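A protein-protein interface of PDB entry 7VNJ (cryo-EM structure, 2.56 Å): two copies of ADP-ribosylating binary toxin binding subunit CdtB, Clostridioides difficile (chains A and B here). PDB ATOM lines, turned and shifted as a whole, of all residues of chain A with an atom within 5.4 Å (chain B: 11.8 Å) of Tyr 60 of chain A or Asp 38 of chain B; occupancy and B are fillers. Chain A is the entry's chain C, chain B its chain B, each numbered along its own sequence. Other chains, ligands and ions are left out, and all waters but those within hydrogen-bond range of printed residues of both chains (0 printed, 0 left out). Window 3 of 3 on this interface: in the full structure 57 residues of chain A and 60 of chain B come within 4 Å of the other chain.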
ATOM      1  N   THR A  20      29.753 -19.003 -28.411  1.00  0.00           N
ATOM      2  CA  THR A  20      28.791 -19.003 -27.314  1.00  0.00           C
ATOM      3  C   THR A  20      29.446 -18.632 -25.989  1.00  0.00           C
ATOM      4  O   THR A  20      28.874 -17.868 -25.204  1.00  0.00           O
ATOM      5  CB  THR A  20      28.113 -20.365 -27.214  1.00  0.00           C
ATOM      6  OG1 THR A  20      27.645 -20.760 -28.508  1.00  0.00           O
ATOM      7  CG2 THR A  20      26.936 -20.301 -26.261  1.00  0.00           C
ATOM      8  N   ASP A  21      30.639 -19.154 -25.720  1.00  0.00           N
ATOM      9  CA  ASP A  21      31.297 -18.938 -24.438  1.00  0.00           C
ATOM     10  C   ASP A  21      32.252 -17.751 -24.443  1.00  0.00           C
ATOM     11  O   ASP A  21      32.879 -17.482 -23.414  1.00  0.00           O
ATOM     12  CB  ASP A  21      32.046 -20.201 -24.009  1.00  0.00           C
ATOM     13  CG  ASP A  21      32.957 -20.731 -25.088  1.00  0.00           C
ATOM     14  OD1 ASP A  21      33.029 -20.106 -26.162  1.00  0.00           O
ATOM     15  OD2 ASP A  21      33.605 -21.771 -24.865  1.00  0.00           O
ATOM     16  N   ASP A  27      32.471 -22.001 -32.340  1.00  0.00           N
ATOM     17  CA  ASP A  27      31.897 -23.236 -31.815  1.00  0.00           C
ATOM     18  C   ASP A  27      32.243 -24.432 -32.690  1.00  0.00           C
ATOM     19  O   ASP A  27      32.611 -25.497 -32.181  1.00  0.00           O
ATOM     20  CB  ASP A  27      30.383 -23.090 -31.686  1.00  0.00           C
ATOM     21  CG  ASP A  27      29.984 -22.124 -30.593  1.00  0.00           C
ATOM     22  OD1 ASP A  27      30.858 -21.741 -29.787  1.00  0.00           O
ATOM     23  OD2 ASP A  27      28.797 -21.745 -30.540  1.00  0.00           O
ATOM     24  N   GLU A  30      35.874 -25.527 -32.133  1.00  0.00           N
ATOM     25  CA  GLU A  30      36.032 -26.330 -30.927  1.00  0.00           C
ATOM     26  C   GLU A  30      35.435 -27.716 -31.097  1.00  0.00           C
ATOM     27  O   GLU A  30      35.949 -28.686 -30.532  1.00  0.00           O
ATOM     28  CB  GLU A  30      35.382 -25.631 -29.733  1.00  0.00           C
ATOM     29  CG  GLU A  30      35.924 -24.252 -29.441  1.00  0.00           C
ATOM     30  CD  GLU A  30      35.629 -23.801 -28.028  1.00  0.00           C
ATOM     31  OE1 GLU A  30      36.178 -24.399 -27.086  1.00  0.00           O
ATOM     32  OE2 GLU A  30      34.843 -22.850 -27.859  1.00  0.00           O
ATOM     33  N   ARG A  31      34.352 -27.828 -31.865  1.00  0.00           N
ATOM     34  CA  ARG A  31      33.689 -29.116 -32.016  1.00  0.00           C
ATOM     35  C   ARG A  31      34.471 -30.045 -32.938  1.00  0.00           C
ATOM     36  O   ARG A  31      34.539 -31.254 -32.694  1.00  0.00           O
ATOM     37  CB  ARG A  31      32.269 -28.901 -32.534  1.00  0.00           C
ATOM     38  CG  ARG A  31      31.282 -29.954 -32.087  1.00  0.00           C
ATOM     39  CD  ARG A  31      29.883 -29.642 -32.585  1.00  0.00           C
ATOM     40  NE  ARG A  31      29.424 -28.328 -32.155  1.00  0.00           N
ATOM     41  CZ  ARG A  31      29.074 -27.350 -32.980  1.00  0.00           C
ATOM     42  NH1 ARG A  31      29.130 -27.500 -34.292  1.00  0.00           N
ATOM     43  NH2 ARG A  31      28.652 -26.196 -32.474  1.00  0.00           N
ATOM     44  N   SER A  58      37.720 -28.893 -27.686  1.00  0.00           N
ATOM     45  CA  SER A  58      37.364 -28.374 -26.373  1.00  0.00           C
ATOM     46  C   SER A  58      35.855 -28.181 -26.296  1.00  0.00           C
ATOM     47  O   SER A  58      35.128 -28.394 -27.269  1.00  0.00           O
ATOM     48  CB  SER A  58      38.112 -27.071 -26.081  1.00  0.00           C
ATOM     49  OG  SER A  58      37.846 -26.098 -27.072  1.00  0.00           O
ATOM     50  N   ASN A  59      35.395 -27.774 -25.117  1.00  0.00           N
ATOM     51  CA  ASN A  59      33.980 -27.549 -24.857  1.00  0.00           C
ATOM     52  C   ASN A  59      33.579 -26.182 -25.396  1.00  0.00           C
ATOM     53  O   ASN A  59      34.119 -25.159 -24.967  1.00  0.00           O
ATOM     54  CB  ASN A  59      33.711 -27.641 -23.357  1.00  0.00           C
ATOM     55  CG  ASN A  59      32.236 -27.656 -23.020  1.00  0.00           C
ATOM     56  OD1 ASN A  59      31.390 -27.331 -23.849  1.00  0.00           O
ATOM     57  ND2 ASN A  59      31.921 -28.033 -21.792  1.00  0.00           N
ATOM     58  N   TYR A  60      32.629 -26.161 -26.327  1.00  0.00           N
ATOM     59  CA  TYR A  60      32.212 -24.898 -26.919  1.00  0.00           C
ATOM     60  C   TYR A  60      31.193 -24.149 -26.072  1.00  0.00           C
ATOM     61  O   TYR A  60      30.872 -23.002 -26.395  1.00  0.00           O
ATOM     62  CB  TYR A  60      31.655 -25.131 -28.327  1.00  0.00           C
ATOM     63  CG  TYR A  60      30.288 -25.766 -28.369  1.00  0.00           C
ATOM     64  CD1 TYR A  60      30.139 -27.141 -28.291  1.00  0.00           C
ATOM     65  CD2 TYR A  60      29.145 -24.991 -28.506  1.00  0.00           C
ATOM     66  CE1 TYR A  60      28.894 -27.724 -28.335  1.00  0.00           C
ATOM     67  CE2 TYR A  60      27.898 -25.565 -28.551  1.00  0.00           C
ATOM     68  CZ  TYR A  60      27.778 -26.931 -28.466  1.00  0.00           C
ATOM     69  OH  TYR A  60      26.532 -27.509 -28.511  1.00  0.00           O
ATOM     70  N   LEU A  61      30.680 -24.759 -25.007  1.00  0.00           N
ATOM     71  CA  LEU A  61      29.774 -24.088 -24.087  1.00  0.00           C
ATOM     72  C   LEU A  61      30.462 -23.625 -22.812  1.00  0.00           C
ATOM     73  O   LEU A  61      29.809 -23.028 -21.953  1.00  0.00           O
ATOM     74  CB  LEU A  61      28.606 -25.009 -23.728  1.00  0.00           C
ATOM     75  CG  LEU A  61      27.552 -25.233 -24.810  1.00  0.00           C
ATOM     76  CD1 LEU A  61      26.367 -25.984 -24.243  1.00  0.00           C
ATOM     77  CD2 LEU A  61      27.113 -23.907 -25.394  1.00  0.00           C
ATOM     78  N   GLU A  62      31.757 -23.883 -22.667  1.00  0.00           N
ATOM     79  CA  GLU A  62      32.495 -23.549 -21.459  1.00  0.00           C
ATOM     80  C   GLU A  62      33.797 -22.869 -21.844  1.00  0.00           C
ATOM     81  O   GLU A  62      34.513 -23.349 -22.727  1.00  0.00           O
ATOM     82  CB  GLU A  62      32.764 -24.802 -20.624  1.00  0.00           C
ATOM     83  CG  GLU A  62      33.694 -24.580 -19.455  1.00  0.00           C
ATOM     84  CD  GLU A  62      33.051 -23.780 -18.341  1.00  0.00           C
ATOM     85  OE1 GLU A  62      31.879 -24.059 -18.007  1.00  0.00           O
ATOM     86  OE2 GLU A  62      33.718 -22.874 -17.799  1.00  0.00           O
ATOM     87  N   GLU A 338      23.855 -31.744 -21.496  1.00  0.00           N
ATOM     88  CA  GLU A 338      24.438 -30.447 -21.807  1.00  0.00           C
ATOM     89  C   GLU A 338      25.935 -30.387 -21.544  1.00  0.00           C
ATOM     90  O   GLU A 338      26.531 -29.314 -21.688  1.00  0.00           O
ATOM     91  CB  GLU A 338      23.729 -29.347 -21.013  1.00  0.00           C
ATOM     92  CG  GLU A 338      22.364 -28.979 -21.562  1.00  0.00           C
ATOM     93  CD  GLU A 338      22.421 -28.518 -23.005  1.00  0.00           C
ATOM     94  OE1 GLU A 338      23.045 -27.471 -23.273  1.00  0.00           O
ATOM     95  OE2 GLU A 338      21.842 -29.203 -23.873  1.00  0.00           O
ATOM     96  N   LYS A 340      29.254 -30.819 -22.937  1.00  0.00           N
ATOM     97  CA  LYS A 340      29.770 -30.906 -24.295  1.00  0.00           C
ATOM     98  C   LYS A 340      31.272 -31.143 -24.348  1.00  0.00           C
ATOM     99  O   LYS A 340      31.873 -30.990 -25.415  1.00  0.00           O
ATOM    100  CB  LYS A 340      29.417 -29.638 -25.072  1.00  0.00           C
ATOM    101  CG  LYS A 340      27.949 -29.280 -25.024  1.00  0.00           C
ATOM    102  CD  LYS A 340      27.111 -30.323 -25.733  1.00  0.00           C
ATOM    103  CE  LYS A 340      25.643 -29.947 -25.721  1.00  0.00           C
ATOM    104  NZ  LYS A 340      24.807 -30.986 -26.375  1.00  0.00           N
ATOM    105  N   ASN B  24      16.931 -13.779 -15.981  1.00  0.00           N
ATOM    106  CA  ASN B  24      17.104 -14.372 -17.305  1.00  0.00           C
ATOM    107  C   ASN B  24      16.131 -15.507 -17.594  1.00  0.00           C
ATOM    108  O   ASN B  24      16.324 -16.236 -18.571  1.00  0.00           O
ATOM    109  CB  ASN B  24      18.535 -14.873 -17.532  1.00  0.00           C
ATOM    110  CG  ASN B  24      19.485 -13.762 -17.910  1.00  0.00           C
ATOM    111  OD1 ASN B  24      19.064 -12.673 -18.296  1.00  0.00           O
ATOM    112  ND2 ASN B  24      20.780 -14.030 -17.800  1.00  0.00           N
ATOM    113  N   TYR B  34      10.548 -25.318 -17.158  1.00  0.00           N
ATOM    114  CA  TYR B  34      11.538 -24.980 -18.167  1.00  0.00           C
ATOM    115  C   TYR B  34      12.749 -25.887 -18.015  1.00  0.00           C
ATOM    116  O   TYR B  34      12.839 -26.693 -17.088  1.00  0.00           O
ATOM    117  CB  TYR B  34      11.956 -23.510 -18.067  1.00  0.00           C
ATOM    118  CG  TYR B  34      12.598 -23.142 -16.747  1.00  0.00           C
ATOM    119  CD1 TYR B  34      11.823 -22.819 -15.645  1.00  0.00           C
ATOM    120  CD2 TYR B  34      13.976 -23.113 -16.608  1.00  0.00           C
ATOM    121  CE1 TYR B  34      12.401 -22.482 -14.442  1.00  0.00           C
ATOM    122  CE2 TYR B  34      14.563 -22.777 -15.407  1.00  0.00           C
ATOM    123  CZ  TYR B  34      13.770 -22.462 -14.329  1.00  0.00           C
ATOM    124  OH  TYR B  34      14.344 -22.125 -13.129  1.00  0.00           O
ATOM    125  N   THR B  35      13.683 -25.740 -18.950  1.00  0.00           N
ATOM    126  CA  THR B  35      14.967 -26.418 -18.886  1.00  0.00           C
ATOM    127  C   THR B  35      15.969 -25.599 -19.685  1.00  0.00           C
ATOM    128  O   THR B  35      15.603 -24.707 -20.449  1.00  0.00           O
ATOM    129  CB  THR B  35      14.879 -27.856 -19.408  1.00  0.00           C
ATOM    130  OG1 THR B  35      16.063 -28.569 -19.039  1.00  0.00           O
ATOM    131  CG2 THR B  35      14.740 -27.871 -20.916  1.00  0.00           C
ATOM    132  N   ILE B  36      17.248 -25.907 -19.494  1.00  0.00           N
ATOM    133  CA  ILE B  36      18.342 -25.152 -20.089  1.00  0.00           C
ATOM    134  C   ILE B  36      18.983 -25.997 -21.179  1.00  0.00           C
ATOM    135  O   ILE B  36      19.326 -27.162 -20.947  1.00  0.00           O
ATOM    136  CB  ILE B  36      19.387 -24.749 -19.036  1.00  0.00           C
ATOM    137  CG1 ILE B  36      18.734 -24.003 -17.873  1.00  0.00           C
ATOM    138  CG2 ILE B  36      20.471 -23.896 -19.668  1.00  0.00           C
ATOM    139  CD1 ILE B  36      18.150 -22.670 -18.251  1.00  0.00           C
ATOM    140  N   LYS B  37      19.144 -25.414 -22.364  1.00  0.00           N
ATOM    141  CA  LYS B  37      19.953 -26.015 -23.416  1.00  0.00           C
ATOM    142  C   LYS B  37      20.653 -24.909 -24.186  1.00  0.00           C
ATOM    143  O   LYS B  37      20.023 -23.918 -24.565  1.00  0.00           O
ATOM    144  CB  LYS B  37      19.112 -26.883 -24.359  1.00  0.00           C
ATOM    145  CG  LYS B  37      17.762 -26.314 -24.712  1.00  0.00           C
ATOM    146  CD  LYS B  37      17.022 -27.253 -25.643  1.00  0.00           C
ATOM    147  CE  LYS B  37      16.792 -28.604 -24.993  1.00  0.00           C
ATOM    148  NZ  LYS B  37      16.057 -29.530 -25.894  1.00  0.00           N
ATOM    149  N   ASP B  38      21.957 -25.087 -24.409  1.00  0.00           N
ATOM    150  CA  ASP B  38      22.813 -24.066 -25.014  1.00  0.00           C
ATOM    151  C   ASP B  38      22.771 -22.765 -24.215  1.00  0.00           C
ATOM    152  O   ASP B  38      22.801 -21.669 -24.778  1.00  0.00           O
ATOM    153  CB  ASP B  38      22.445 -23.820 -26.479  1.00  0.00           C
ATOM    154  CG  ASP B  38      22.863 -24.961 -27.381  1.00  0.00           C
ATOM    155  OD1 ASP B  38      23.644 -25.821 -26.928  1.00  0.00           O
ATOM    156  OD2 ASP B  38      22.414 -24.999 -28.544  1.00  0.00           O
ATOM    157  N   LEU B  39      22.693 -22.897 -22.890  1.00  0.00           N
ATOM    158  CA  LEU B  39      22.748 -21.768 -21.960  1.00  0.00           C
ATOM    159  C   LEU B  39      21.586 -20.799 -22.155  1.00  0.00           C
ATOM    160  O   LEU B  39      21.692 -19.616 -21.827  1.00  0.00           O
ATOM    161  CB  LEU B  39      24.081 -21.025 -22.066  1.00  0.00           C
ATOM    162  CG  LEU B  39      25.336 -21.870 -21.858  1.00  0.00           C
ATOM    163  CD1 LEU B  39      26.576 -21.072 -22.209  1.00  0.00           C
ATOM    164  CD2 LEU B  39      25.406 -22.373 -20.430  1.00  0.00           C
ATOM    165  N   ILE B  40      20.467 -21.283 -22.687  1.00  0.00           N
ATOM    166  CA  ILE B  40      19.267 -20.475 -22.870  1.00  0.00           C
ATOM    167  C   ILE B  40      18.068 -21.285 -22.402  1.00  0.00           C
ATOM    168  O   ILE B  40      17.890 -22.434 -22.819  1.00  0.00           O
ATOM    169  CB  ILE B  40      19.089 -20.036 -24.336  1.00  0.00           C
ATOM    170  CG1 ILE B  40      20.136 -18.985 -24.703  1.00  0.00           C
ATOM    171  CG2 ILE B  40      17.693 -19.490 -24.566  1.00  0.00           C
ATOM    172  CD1 ILE B  40      19.913 -18.344 -26.052  1.00  0.00           C
ATOM    173  N   ALA B  41      17.249 -20.689 -21.539  1.00  0.00           N
ATOM    174  CA  ALA B  41      16.072 -21.373 -21.024  1.00  0.00           C
ATOM    175  C   ALA B  41      15.031 -21.556 -22.120  1.00  0.00           C
ATOM    176  O   ALA B  41      14.767 -20.645 -22.908  1.00  0.00           O
ATOM    177  CB  ALA B  41      15.473 -20.591 -19.858  1.00  0.00           C
ATOM    178  N   VAL B  42      14.431 -22.745 -22.162  1.00  0.00           N
ATOM    179  CA  VAL B  42      13.416 -23.079 -23.150  1.00  0.00           C
ATOM    180  C   VAL B  42      12.204 -23.660 -22.435  1.00  0.00           C
ATOM    181  O   VAL B  42      12.287 -24.132 -21.301  1.00  0.00           O
ATOM    182  CB  VAL B  42      13.932 -24.072 -24.214  1.00  0.00           C
ATOM    183  CG1 VAL B  42      15.105 -23.480 -24.970  1.00  0.00           C
ATOM    184  CG2 VAL B  42      14.324 -25.381 -23.566  1.00  0.00           C
ATOM    185  N   LYS B  43      11.064 -23.613 -23.121  1.00  0.00           N
ATOM    186  CA  LYS B  43       9.837 -24.176 -22.577  1.00  0.00           C
ATOM    187  C   LYS B  43       9.945 -25.690 -22.470  1.00  0.00           C
ATOM    188  O   LYS B  43      10.491 -26.354 -23.353  1.00  0.00           O
ATOM    189  CB  LYS B  43       8.646 -23.802 -23.455  1.00  0.00           C
ATOM    190  CG  LYS B  43       7.887 -22.582 -22.984  1.00  0.00           C
ATOM    191  CD  LYS B  43       6.801 -22.198 -23.972  1.00  0.00           C
ATOM    192  CE  LYS B  43       5.916 -23.385 -24.306  1.00  0.00           C
ATOM    193  NZ  LYS B  43       4.640 -22.969 -24.950  1.00  0.00           N
ATOM    194  N   PHE B  48      11.440 -34.214 -23.593  1.00  0.00           N
ATOM    195  CA  PHE B  48      12.803 -33.895 -23.183  1.00  0.00           C
ATOM    196  C   PHE B  48      13.333 -34.883 -22.153  1.00  0.00           C
ATOM    197  O   PHE B  48      14.549 -35.076 -22.055  1.00  0.00           O
ATOM    198  CB  PHE B  48      12.867 -32.476 -22.622  1.00  0.00           C
ATOM    199  CG  PHE B  48      12.756 -31.404 -23.663  1.00  0.00           C
ATOM    200  CD1 PHE B  48      12.817 -31.715 -25.009  1.00  0.00           C
ATOM    201  CD2 PHE B  48      12.592 -30.082 -23.294  1.00  0.00           C
ATOM    202  CE1 PHE B  48      12.714 -30.728 -25.964  1.00  0.00           C
ATOM    203  CE2 PHE B  48      12.489 -29.091 -24.246  1.00  0.00           C
ATOM    204  CZ  PHE B  48      12.549 -29.415 -25.582  1.00  0.00           C
ATOM    205  N   GLN B  51      15.828 -37.731 -23.179  1.00  0.00           N
ATOM    206  CA  GLN B  51      17.225 -37.414 -23.434  1.00  0.00           C
ATOM    207  C   GLN B  51      17.985 -37.008 -22.179  1.00  0.00           C
ATOM    208  O   GLN B  51      19.149 -36.608 -22.281  1.00  0.00           O
ATOM    209  CB  GLN B  51      17.328 -36.307 -24.482  1.00  0.00           C
ATOM    210  CG  GLN B  51      16.613 -36.631 -25.779  1.00  0.00           C
ATOM    211  CD  GLN B  51      16.095 -35.398 -26.485  1.00  0.00           C
ATOM    212  OE1 GLN B  51      16.708 -34.334 -26.431  1.00  0.00           O
ATOM    213  NE2 GLN B  51      14.955 -35.533 -27.151  1.00  0.00           N
ATOM    214  N   TYR B  53      16.972 -34.613 -19.777  1.00  0.00           N
ATOM    215  CA  TYR B  53      16.745 -33.268 -19.277  1.00  0.00           C
ATOM    216  C   TYR B  53      15.848 -33.295 -18.046  1.00  0.00           C
ATOM    217  O   TYR B  53      15.030 -34.200 -17.863  1.00  0.00           O
ATOM    218  CB  TYR B  53      16.118 -32.392 -20.357  1.00  0.00           C
ATOM    219  CG  TYR B  53      17.080 -31.991 -21.445  1.00  0.00           C
ATOM    220  CD1 TYR B  53      17.966 -30.943 -21.262  1.00  0.00           C
ATOM    221  CD2 TYR B  53      17.103 -32.661 -22.659  1.00  0.00           C
ATOM    222  CE1 TYR B  53      18.847 -30.572 -22.252  1.00  0.00           C
ATOM    223  CE2 TYR B  53      17.980 -32.296 -23.656  1.00  0.00           C
ATOM    224  CZ  TYR B  53      18.851 -31.251 -23.447  1.00  0.00           C
ATOM    225  OH  TYR B  53      19.729 -30.883 -24.437  1.00  0.00           O
ATOM    226  N   LYS B  54      16.011 -32.286 -17.197  1.00  0.00           N
ATOM    227  CA  LYS B  54      15.220 -32.132 -15.988  1.00  0.00           C
ATOM    228  C   LYS B  54      14.305 -30.924 -16.116  1.00  0.00           C
ATOM    229  O   LYS B  54      14.651 -29.927 -16.756  1.00  0.00           O
ATOM    230  CB  LYS B  54      16.115 -31.972 -14.757  1.00  0.00           C
ATOM    231  CG  LYS B  54      17.097 -33.105 -14.553  1.00  0.00           C
ATOM    232  CD  LYS B  54      16.623 -34.052 -13.469  1.00  0.00           C
ATOM    233  CE  LYS B  54      17.352 -35.380 -13.540  1.00  0.00           C
ATOM    234  NZ  LYS B  54      18.819 -35.218 -13.352  1.00  0.00           N
ATOM    235  N   TYR B  56      12.358 -27.813 -14.403  1.00  0.00           N
ATOM    236  CA  TYR B  56      12.570 -26.903 -13.288  1.00  0.00           C
ATOM    237  C   TYR B  56      11.409 -25.928 -13.173  1.00  0.00           C
ATOM    238  O   TYR B  56      10.864 -25.472 -14.181  1.00  0.00           O
ATOM    239  CB  TYR B  56      13.872 -26.115 -13.455  1.00  0.00           C
ATOM    240  CG  TYR B  56      15.112 -26.969 -13.511  1.00  0.00           C
ATOM    241  CD1 TYR B  56      15.312 -27.994 -12.603  1.00  0.00           C
ATOM    242  CD2 TYR B  56      16.086 -26.745 -14.469  1.00  0.00           C
ATOM    243  CE1 TYR B  56      16.443 -28.773 -12.651  1.00  0.00           C
ATOM    244  CE2 TYR B  56      17.220 -27.520 -14.524  1.00  0.00           C
ATOM    245  CZ  TYR B  56      17.395 -28.532 -13.611  1.00  0.00           C
ATOM    246  OH  TYR B  56      18.524 -29.310 -13.658  1.00  0.00           O
ATOM    247  N   TYR B  73      18.919 -18.953 -12.617  1.00  0.00           N
ATOM    248  CA  TYR B  73      19.580 -19.267 -13.879  1.00  0.00           C
ATOM    249  C   TYR B  73      20.938 -19.912 -13.648  1.00  0.00           C
ATOM    250  O   TYR B  73      21.295 -20.873 -14.336  1.00  0.00           O
ATOM    251  CB  TYR B  73      19.733 -18.009 -14.729  1.00  0.00           C
ATOM    252  CG  TYR B  73      20.519 -18.253 -15.992  1.00  0.00           C
ATOM    253  CD1 TYR B  73      19.919 -18.827 -17.103  1.00  0.00           C
ATOM    254  CD2 TYR B  73      21.865 -17.929 -16.070  1.00  0.00           C
ATOM    255  CE1 TYR B  73      20.634 -19.061 -18.256  1.00  0.00           C
ATOM    256  CE2 TYR B  73      22.587 -18.161 -17.216  1.00  0.00           C
ATOM    257  CZ  TYR B  73      21.968 -18.727 -18.308  1.00  0.00           C
ATOM    258  OH  TYR B  73      22.686 -18.958 -19.456  1.00  0.00           O
ATOM    259  N   ALA B  76      20.255 -23.572 -12.449  1.00  0.00           N
ATOM    260  CA  ALA B  76      19.692 -24.438 -13.479  1.00  0.00           C
ATOM    261  C   ALA B  76      20.668 -24.676 -14.621  1.00  0.00           C
ATOM    262  O   ALA B  76      20.669 -25.757 -15.218  1.00  0.00           O
ATOM    263  CB  ALA B  76      18.391 -23.842 -14.012  1.00  0.00           C
ATOM    264  N   SER B  77      21.498 -23.687 -14.941  1.00  0.00           N
ATOM    265  CA  SER B  77      22.431 -23.791 -16.052  1.00  0.00           C
ATOM    266  C   SER B  77      23.741 -24.468 -15.676  1.00  0.00           C
ATOM    267  O   SER B  77      24.491 -24.862 -16.573  1.00  0.00           O
ATOM    268  CB  SER B  77      22.720 -22.398 -16.609  1.00  0.00           C
ATOM    269  OG  SER B  77      23.806 -22.427 -17.512  1.00  0.00           O
ATOM    270  N   GLY B  78      23.929 -24.730 -14.378  1.00  0.00           N
ATOM    271  CA  GLY B  78      25.170 -25.373 -13.905  1.00  0.00           C
ATOM    272  C   GLY B  78      26.336 -24.425 -14.077  1.00  0.00           C
ATOM    273  O   GLY B  78      27.486 -24.898 -14.078  1.00  0.00           O
ATOM    274  N   SER B  79      26.044 -23.128 -14.204  1.00  0.00           N
ATOM    275  CA  SER B  79      27.103 -22.106 -14.408  1.00  0.00           C
ATOM    276  C   SER B  79      27.658 -21.643 -13.057  1.00  0.00           C
ATOM    277  O   SER B  79      27.780 -20.419 -12.863  1.00  0.00           O
ATOM    278  CB  SER B  79      26.568 -20.949 -15.206  1.00  0.00           C
ATOM    279  OG  SER B  79      26.340 -21.332 -16.554  1.00  0.00           O
ATOM    280  N   LYS B  82      31.924 -26.138 -10.265  1.00  0.00           N
ATOM    281  CA  LYS B  82      31.652 -27.492 -10.814  1.00  0.00           C
ATOM    282  C   LYS B  82      31.677 -28.528  -9.684  1.00  0.00           C
ATOM    283  O   LYS B  82      31.248 -29.671  -9.936  1.00  0.00           O
ATOM    284  CB  LYS B  82      32.663 -27.852 -11.906  1.00  0.00           C
ATOM    285  CG  LYS B  82      32.589 -27.014 -13.176  1.00  0.00           C
ATOM    286  CD  LYS B  82      31.181 -26.777 -13.673  1.00  0.00           C
ATOM    287  CE  LYS B  82      31.057 -25.517 -14.505  1.00  0.00           C
ATOM    288  NZ  LYS B  82      30.073 -25.676 -15.602  1.00  0.00           N
ATOM    289  N   ARG B  89      21.177 -28.245  -8.463  1.00  0.00           N
ATOM    290  CA  ARG B  89      21.015 -27.459  -9.676  1.00  0.00           C
ATOM    291  C   ARG B  89      19.591 -26.964  -9.873  1.00  0.00           C
ATOM    292  O   ARG B  89      19.392 -25.925 -10.507  1.00  0.00           O
ATOM    293  CB  ARG B  89      21.455 -28.268 -10.896  1.00  0.00           C
ATOM    294  CG  ARG B  89      22.926 -28.102 -11.216  1.00  0.00           C
ATOM    295  CD  ARG B  89      23.404 -29.126 -12.213  1.00  0.00           C
ATOM    296  NE  ARG B  89      22.925 -28.838 -13.557  1.00  0.00           N
ATOM    297  CZ  ARG B  89      23.681 -28.881 -14.644  1.00  0.00           C
ATOM    298  NH1 ARG B  89      24.966 -29.189 -14.580  1.00  0.00           N
ATOM    299  NH2 ARG B  89      23.136 -28.607 -15.825  1.00  0.00           N
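The backbone carbonyl oxygen of Phe 48 of chain B lies within hydrogen-bond range of the backbone NH of Tyr 53 of chain B (3.4 Å). The side-chain hydroxyl (OH) of Tyr 73 of chain B sits at hydrogen-bond distance from the backbone carbonyl oxygen (O) of Leu 39 of chain B, 2.7 Å away. O of Gly 78 of chain B is in hydrogen-bond range of NZ of Lys 82 of chain B (3.1 Å). N of Leu 61 of chain A lies within hydrogen-bond range of OD1 of Asn 59 of chain A (2.9 Å).
Of chain B, only Asp 38 (3.7 Å) comes within 4 Å of Tyr 60 of chain A. No residue of chain B comes within 4 Å of Thr 20 of chain A. No residue of chain B comes within 4 Å of Asp 21 of chain A. No residue of chain B comes within 4 Å of Glu 30 of chain A. No residue of chain B comes within 4 Å of Arg 31 of chain A. No residue of chain B comes within 4 Å of Asn 59 of chain A. Of chain B, only Asp 38 (3.8 Å) and Leu 39 (3.8 Å) come within 4 Å of Leu 61 of chain A. Of chain B, only Ile 36 (3.6 Å), Lys 37 (3.4 Å), Asp 38 (2.9 Å) and Tyr 53 (2.8 Å) come within 4 Å of Glu 338 of chain A. No residue of chain B comes within 4 Å of Lys 340 of chain A. Printed residues of chain A within 4 Å of Lys 82 of chain B: Glu 62. Of the printed residues of chain A, Leu 39 of chain B touches Leu 61. Of the printed residues of chain A, Lys 37 of chain B touches Glu 338 (3.4 Å). Ile 40 of chain B touches none of the printed residues of chain A. The nearest residue of chain B that does not touch Tyr 60 of chain A is Leu 39 of chain B (6.3 Å).
Among the printed residues, merely in contact across the chains: Tyr 60 of chain A with Asp 38 of chain B (3.7 Å), Leu 61 of chain A with Asp 38 of chain B (3.8 Å), Leu 61 of chain A with Leu 39 of chain B (3.8 Å), Glu 338 of chain A with Ile 36 of chain B (3.6 Å) and Glu 338 of chain A with Lys 37 of chain B (3.4 Å).
No position is printed for both chains. Of the 8 pairs that touch across the chains among the printed residues, none has its exchanged pair printed and touching as well.
Hydrophobic or aromatic side chains of chain A within 4 Å of the printed part of chain B: Tyr 60 and Leu 61.
The side-chain amino group of Lys 82 of chain B lies within salt-bridge range of the side-chain carboxylate of Glu 62 of chain A (3.4 Å). The side-chain carboxylate (OE2) of Glu 338 of chain A is in hydrogen-bond range of the side-chain hydroxyl (OH) of Tyr 53 of chain B, at 2.8 Å. OE1 of Glu 338 of chain A lies within hydrogen-bond range of N of Asp 38 of chain B, at 2.9 Å.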
